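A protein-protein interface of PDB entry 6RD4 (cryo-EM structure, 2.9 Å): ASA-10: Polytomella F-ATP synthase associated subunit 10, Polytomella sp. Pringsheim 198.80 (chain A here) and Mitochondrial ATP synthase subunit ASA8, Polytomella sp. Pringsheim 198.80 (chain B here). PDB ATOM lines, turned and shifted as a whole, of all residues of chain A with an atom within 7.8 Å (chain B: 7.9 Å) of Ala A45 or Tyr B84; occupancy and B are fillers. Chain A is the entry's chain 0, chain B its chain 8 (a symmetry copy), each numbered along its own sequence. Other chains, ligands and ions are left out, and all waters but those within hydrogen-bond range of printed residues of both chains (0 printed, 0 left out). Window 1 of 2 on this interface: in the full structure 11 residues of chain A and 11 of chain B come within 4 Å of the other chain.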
ATOM      1  N   ILE A  42     -12.665  -2.824 -13.068  1.00  0.00           N
ATOM      2  CA  ILE A  42     -11.999  -2.852 -11.780  1.00  0.00           C
ATOM      3  C   ILE A  42     -10.549  -3.249 -11.993  1.00  0.00           C
ATOM      4  O   ILE A  42     -10.120  -3.564 -13.101  1.00  0.00           O
ATOM      5  CB  ILE A  42     -12.702  -3.810 -10.816  1.00  0.00           C
ATOM      6  CG1 ILE A  42     -12.653  -5.226 -11.358  1.00  0.00           C
ATOM      7  CG2 ILE A  42     -14.119  -3.372 -10.635  1.00  0.00           C
ATOM      8  CD1 ILE A  42     -13.479  -6.191 -10.577  1.00  0.00           C
ATOM      9  N   SER A  43      -9.780  -3.209 -10.915  1.00  0.00           N
ATOM     10  CA  SER A  43      -8.389  -3.620 -10.974  1.00  0.00           C
ATOM     11  C   SER A  43      -8.293  -5.136 -11.025  1.00  0.00           C
ATOM     12  O   SER A  43      -9.246  -5.856 -10.725  1.00  0.00           O
ATOM     13  CB  SER A  43      -7.633  -3.094  -9.768  1.00  0.00           C
ATOM     14  OG  SER A  43      -8.317  -3.451  -8.584  1.00  0.00           O
ATOM     15  N   ASN A  44      -7.118  -5.628 -11.417  1.00  0.00           N
ATOM     16  CA  ASN A  44      -6.911  -7.068 -11.453  1.00  0.00           C
ATOM     17  C   ASN A  44      -6.869  -7.660 -10.055  1.00  0.00           C
ATOM     18  O   ASN A  44      -7.262  -8.815  -9.859  1.00  0.00           O
ATOM     19  CB  ASN A  44      -5.623  -7.393 -12.197  1.00  0.00           C
ATOM     20  CG  ASN A  44      -5.825  -7.516 -13.677  1.00  0.00           C
ATOM     21  OD1 ASN A  44      -5.019  -7.035 -14.469  1.00  0.00           O
ATOM     22  ND2 ASN A  44      -6.905  -8.177 -14.068  1.00  0.00           N
ATOM     23  N   ALA A  45      -6.416  -6.880  -9.074  1.00  0.00           N
ATOM     24  CA  ALA A  45      -6.389  -7.345  -7.697  1.00  0.00           C
ATOM     25  C   ALA A  45      -7.790  -7.524  -7.134  1.00  0.00           C
ATOM     26  O   ALA A  45      -8.002  -8.371  -6.267  1.00  0.00           O
ATOM     27  CB  ALA A  45      -5.594  -6.366  -6.842  1.00  0.00           C
ATOM     28  N   GLU A  46      -8.751  -6.737  -7.606  1.00  0.00           N
ATOM     29  CA  GLU A  46     -10.130  -6.931  -7.195  1.00  0.00           C
ATOM     30  C   GLU A  46     -10.787  -8.072  -7.946  1.00  0.00           C
ATOM     31  O   GLU A  46     -11.618  -8.780  -7.379  1.00  0.00           O
ATOM     32  CB  GLU A  46     -10.924  -5.647  -7.394  1.00  0.00           C
ATOM     33  CG  GLU A  46     -12.311  -5.680  -6.794  1.00  0.00           C
ATOM     34  CD  GLU A  46     -13.059  -4.392  -6.996  1.00  0.00           C
ATOM     35  OE1 GLU A  46     -12.444  -3.421  -7.474  1.00  0.00           O
ATOM     36  OE2 GLU A  46     -14.256  -4.349  -6.666  1.00  0.00           O
ATOM     37  N   TYR A  47     -10.428  -8.273  -9.212  1.00  0.00           N
ATOM     38  CA  TYR A  47     -11.082  -9.317  -9.984  1.00  0.00           C
ATOM     39  C   TYR A  47     -10.622 -10.697  -9.550  1.00  0.00           C
ATOM     40  O   TYR A  47     -11.411 -11.648  -9.572  1.00  0.00           O
ATOM     41  CB  TYR A  47     -10.830  -9.121 -11.482  1.00  0.00           C
ATOM     42  CG  TYR A  47     -11.681 -10.034 -12.324  1.00  0.00           C
ATOM     43  CD1 TYR A  47     -12.997  -9.723 -12.587  1.00  0.00           C
ATOM     44  CD2 TYR A  47     -11.180 -11.221 -12.821  1.00  0.00           C
ATOM     45  CE1 TYR A  47     -13.781 -10.553 -13.331  1.00  0.00           C
ATOM     46  CE2 TYR A  47     -11.964 -12.060 -13.557  1.00  0.00           C
ATOM     47  CZ  TYR A  47     -13.265 -11.719 -13.808  1.00  0.00           C
ATOM     48  OH  TYR A  47     -14.058 -12.551 -14.551  1.00  0.00           O
ATOM     49  N   ASN A  48      -9.358 -10.827  -9.162  1.00  0.00           N
ATOM     50  CA  ASN A  48      -8.844 -12.107  -8.708  1.00  0.00           C
ATOM     51  C   ASN A  48      -9.274 -12.438  -7.292  1.00  0.00           C
ATOM     52  O   ASN A  48      -9.219 -13.605  -6.903  1.00  0.00           O
ATOM     53  CB  ASN A  48      -7.322 -12.104  -8.795  1.00  0.00           C
ATOM     54  CG  ASN A  48      -6.824 -11.943 -10.206  1.00  0.00           C
ATOM     55  OD1 ASN A  48      -5.852 -11.240 -10.453  1.00  0.00           O
ATOM     56  ND2 ASN A  48      -7.477 -12.610 -11.141  1.00  0.00           N
ATOM     57  N   ALA A  49      -9.708 -11.446  -6.523  1.00  0.00           N
ATOM     58  CA  ALA A  49     -10.082 -11.639  -5.137  1.00  0.00           C
ATOM     59  C   ALA A  49     -11.576 -11.781  -4.920  1.00  0.00           C
ATOM     60  O   ALA A  49     -11.988 -12.155  -3.823  1.00  0.00           O
ATOM     61  CB  ALA A  49      -9.574 -10.473  -4.292  1.00  0.00           C
ATOM     62  N   THR A  50     -12.386 -11.501  -5.919  1.00  0.00           N
ATOM     63  CA  THR A  50     -13.827 -11.462  -5.752  1.00  0.00           C
ATOM     64  C   THR A  50     -14.454 -12.732  -6.301  1.00  0.00           C
ATOM     65  O   THR A  50     -14.049 -13.204  -7.364  1.00  0.00           O
ATOM     66  CB  THR A  50     -14.402 -10.254  -6.489  1.00  0.00           C
ATOM     67  OG1 THR A  50     -13.594  -9.106  -6.217  1.00  0.00           O
ATOM     68  CG2 THR A  50     -15.780  -9.944  -6.024  1.00  0.00           C
ATOM     69  N   HIS A  81     -21.990  -0.667   0.958  1.00  0.00           N
ATOM     70  CA  HIS A  81     -21.418   0.482   1.651  1.00  0.00           C
ATOM     71  C   HIS A  81     -22.498   1.476   2.049  1.00  0.00           C
ATOM     72  O   HIS A  81     -22.344   2.691   1.898  1.00  0.00           O
ATOM     73  CB  HIS A  81     -20.346   1.143   0.797  1.00  0.00           C
ATOM     74  CG  HIS A  81     -18.990   0.540   0.979  1.00  0.00           C
ATOM     75  ND1 HIS A  81     -17.885   0.951   0.266  1.00  0.00           N
ATOM     76  CD2 HIS A  81     -18.560  -0.448   1.801  1.00  0.00           C
ATOM     77  CE1 HIS A  81     -16.836   0.240   0.637  1.00  0.00           C
ATOM     78  NE2 HIS A  81     -17.218  -0.614   1.567  1.00  0.00           N
ATOM     79  N   ALA B  72     -12.657 -16.238   1.931  1.00  0.00           N
ATOM     80  CA  ALA B  72     -11.640 -15.260   2.271  1.00  0.00           C
ATOM     81  C   ALA B  72     -12.086 -13.829   2.037  1.00  0.00           C
ATOM     82  O   ALA B  72     -11.437 -12.909   2.534  1.00  0.00           O
ATOM     83  CB  ALA B  72     -10.364 -15.525   1.479  1.00  0.00           C
ATOM     84  N   TYR B  73     -13.149 -13.612   1.270  1.00  0.00           N
ATOM     85  CA  TYR B  73     -13.646 -12.259   1.048  1.00  0.00           C
ATOM     86  C   TYR B  73     -14.502 -11.798   2.207  1.00  0.00           C
ATOM     87  O   TYR B  73     -14.366 -10.664   2.668  1.00  0.00           O
ATOM     88  CB  TYR B  73     -14.455 -12.201  -0.238  1.00  0.00           C
ATOM     89  CG  TYR B  73     -14.665 -10.833  -0.814  1.00  0.00           C
ATOM     90  CD1 TYR B  73     -13.726 -10.265  -1.641  1.00  0.00           C
ATOM     91  CD2 TYR B  73     -15.825 -10.135  -0.572  1.00  0.00           C
ATOM     92  CE1 TYR B  73     -13.921  -9.032  -2.189  1.00  0.00           C
ATOM     93  CE2 TYR B  73     -16.025  -8.897  -1.115  1.00  0.00           C
ATOM     94  CZ  TYR B  73     -15.066  -8.353  -1.923  1.00  0.00           C
ATOM     95  OH  TYR B  73     -15.255  -7.115  -2.473  1.00  0.00           O
ATOM     96  N   ALA B  76     -12.693 -10.685   5.380  1.00  0.00           N
ATOM     97  CA  ALA B  76     -12.052  -9.384   5.436  1.00  0.00           C
ATOM     98  C   ALA B  76     -13.039  -8.244   5.600  1.00  0.00           C
ATOM     99  O   ALA B  76     -12.695  -7.238   6.214  1.00  0.00           O
ATOM    100  CB  ALA B  76     -11.207  -9.145   4.184  1.00  0.00           C
ATOM    101  N   ILE B  77     -14.256  -8.369   5.074  1.00  0.00           N
ATOM    102  CA  ILE B  77     -15.265  -7.353   5.339  1.00  0.00           C
ATOM    103  C   ILE B  77     -16.032  -7.615   6.632  1.00  0.00           C
ATOM    104  O   ILE B  77     -16.757  -6.724   7.096  1.00  0.00           O
ATOM    105  CB  ILE B  77     -16.250  -7.202   4.167  1.00  0.00           C
ATOM    106  CG1 ILE B  77     -17.314  -8.291   4.192  1.00  0.00           C
ATOM    107  CG2 ILE B  77     -15.508  -7.227   2.860  1.00  0.00           C
ATOM    108  CD1 ILE B  77     -18.409  -8.088   3.167  1.00  0.00           C
ATOM    109  N   LYS B  81     -10.832  -5.296   7.149  1.00  0.00           N
ATOM    110  CA  LYS B  81      -9.725  -5.108   6.230  1.00  0.00           C
ATOM    111  C   LYS B  81     -10.244  -4.975   4.807  1.00  0.00           C
ATOM    112  O   LYS B  81     -11.377  -5.339   4.499  1.00  0.00           O
ATOM    113  CB  LYS B  81      -8.726  -6.265   6.315  1.00  0.00           C
ATOM    114  CG  LYS B  81      -8.098  -6.441   7.677  1.00  0.00           C
ATOM    115  CD  LYS B  81      -7.072  -7.563   7.669  1.00  0.00           C
ATOM    116  CE  LYS B  81      -7.099  -8.365   8.968  1.00  0.00           C
ATOM    117  NZ  LYS B  81      -8.458  -8.852   9.320  1.00  0.00           N
ATOM    118  N   THR B  82      -9.416  -4.422   3.960  1.00  0.00           N
ATOM    119  CA  THR B  82      -9.768  -4.421   2.554  1.00  0.00           C
ATOM    120  C   THR B  82      -9.400  -5.770   1.938  1.00  0.00           C
ATOM    121  O   THR B  82      -8.335  -6.322   2.227  1.00  0.00           O
ATOM    122  CB  THR B  82      -9.073  -3.269   1.821  1.00  0.00           C
ATOM    123  OG1 THR B  82      -9.275  -3.396   0.408  1.00  0.00           O
ATOM    124  CG2 THR B  82      -7.580  -3.191   2.150  1.00  0.00           C
ATOM    125  N   PRO B  83     -10.280  -6.350   1.121  1.00  0.00           N
ATOM    126  CA  PRO B  83     -10.092  -7.739   0.699  1.00  0.00           C
ATOM    127  C   PRO B  83      -9.066  -7.940  -0.400  1.00  0.00           C
ATOM    128  O   PRO B  83      -8.871  -9.079  -0.831  1.00  0.00           O
ATOM    129  CB  PRO B  83     -11.487  -8.131   0.217  1.00  0.00           C
ATOM    130  CG  PRO B  83     -12.400  -7.107   0.780  1.00  0.00           C
ATOM    131  CD  PRO B  83     -11.621  -5.868   0.782  1.00  0.00           C
ATOM    132  N   TYR B  84      -8.404  -6.888  -0.858  1.00  0.00           N
ATOM    133  CA  TYR B  84      -7.377  -7.013  -1.877  1.00  0.00           C
ATOM    134  C   TYR B  84      -6.372  -5.896  -1.663  1.00  0.00           C
ATOM    135  O   TYR B  84      -6.524  -5.064  -0.768  1.00  0.00           O
ATOM    136  CB  TYR B  84      -7.985  -6.975  -3.275  1.00  0.00           C
ATOM    137  CG  TYR B  84      -9.071  -5.953  -3.457  1.00  0.00           C
ATOM    138  CD1 TYR B  84     -10.402  -6.285  -3.283  1.00  0.00           C
ATOM    139  CD2 TYR B  84      -8.766  -4.664  -3.847  1.00  0.00           C
ATOM    140  CE1 TYR B  84     -11.386  -5.362  -3.461  1.00  0.00           C
ATOM    141  CE2 TYR B  84      -9.752  -3.732  -4.028  1.00  0.00           C
ATOM    142  CZ  TYR B  84     -11.056  -4.088  -3.831  1.00  0.00           C
ATOM    143  OH  TYR B  84     -12.041  -3.155  -4.010  1.00  0.00           O
ATOM    144  N   THR B  85      -5.347  -5.860  -2.508  1.00  0.00           N
ATOM    145  CA  THR B  85      -4.236  -4.939  -2.316  1.00  0.00           C
ATOM    146  C   THR B  85      -4.468  -3.571  -2.953  1.00  0.00           C
ATOM    147  O   THR B  85      -3.495  -2.843  -3.187  1.00  0.00           O
ATOM    148  CB  THR B  85      -2.941  -5.563  -2.842  1.00  0.00           C
ATOM    149  OG1 THR B  85      -1.833  -4.723  -2.500  1.00  0.00           O
ATOM    150  CG2 THR B  85      -2.987  -5.799  -4.353  1.00  0.00           C
ATOM    151  N   ALA B  86      -5.734  -3.205  -3.196  1.00  0.00           N
ATOM    152  CA  ALA B  86      -6.148  -1.907  -3.752  1.00  0.00           C
ATOM    153  C   ALA B  86      -5.519  -1.640  -5.120  1.00  0.00           C
ATOM    154  O   ALA B  86      -5.155  -0.512  -5.450  1.00  0.00           O
ATOM    155  CB  ALA B  86      -5.871  -0.752  -2.782  1.00  0.00           C
ATOM    156  N   GLY B  87      -5.382  -2.690  -5.920  1.00  0.00           N
ATOM    157  CA  GLY B  87      -5.001  -2.523  -7.306  1.00  0.00           C
ATOM    158  C   GLY B  87      -3.534  -2.262  -7.564  1.00  0.00           C
ATOM    159  O   GLY B  87      -2.840  -3.109  -8.134  1.00  0.00           O
ATOM    160  N   GLY B  88      -3.045  -1.092  -7.155  1.00  0.00           N
ATOM    161  CA  GLY B  88      -1.689  -0.655  -7.442  1.00  0.00           C
ATOM    162  C   GLY B  88      -1.622   0.719  -8.078  1.00  0.00           C
ATOM    163  O   GLY B  88      -0.533   1.291  -8.192  1.00  0.00           O
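Among the printed residues, merely in contact across the chains: Ala A45 with Tyr B84 (3.3 Å), Ala A49 with Tyr B73 (3.4 Å), Ala A45 with Thr B85 (3.6 Å), Ser A43 with Gly B87 (3.6 Å), Ala A45 with Gly B87 (3.8 Å), Ala A49 with Pro B83 (3.8 Å) and Ala A49 with Tyr B84 (3.97 Å).
Of the 10 printed residues of chain A, 4 touch a printed residue of chain B.
Hydrophobic or aromatic side chains of chain A within 4 Å of the printed part of chain B: Ala A45 and Ala A49.
Along chain A the printed residues that touch a printed residue of chain B span positions 43 to 49.
Of the 12 printed residues of chain B, 5 touch a printed residue of chain A.
Among the printed residues, 8 pairs touch across the chains.
OE1 of Glu A46 sits close to OH of Tyr B84.
Ala A45 touches just these residues of chain B: Tyr B84 (3.3 Å), Thr B85 (3.6 Å) and Gly B87 (3.8 Å).
Tyr B84 touches just these residues of chain A: Ala A45 (3.3 Å), Glu A46 (3.4 Å) and Ala A49 (3.97 Å).
Glu A46 touches one residue of chain B.
Of the printed residues of chain A, Thr B85 touches Ala A45.
Printed residues of chain B within 4 Å of Ala A49: Tyr B73 (3.4 Å), Pro B83 (3.8 Å) and Tyr B84 (3.97 Å).
Printed residues of chain A within 4 Å of Gly B87: Ser A43 (3.6 Å) and Ala A45 (3.8 Å).
Printed residues of chain B within 4 Å of Ser A43: Gly B87.
Ile A42 touches none of the printed residues of chain B.
The nearest residue of chain A that does not touch Tyr B84 is Ser A43 (4.8 Å).
N of Glu A46 is in hydrogen-bond range of OG of Ser A43, 3.5 Å away.
The side-chain hydroxyl of Thr B82 is in hydrogen-bond range of the backbone carbonyl oxygen of Tyr B84 (3.4 Å).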
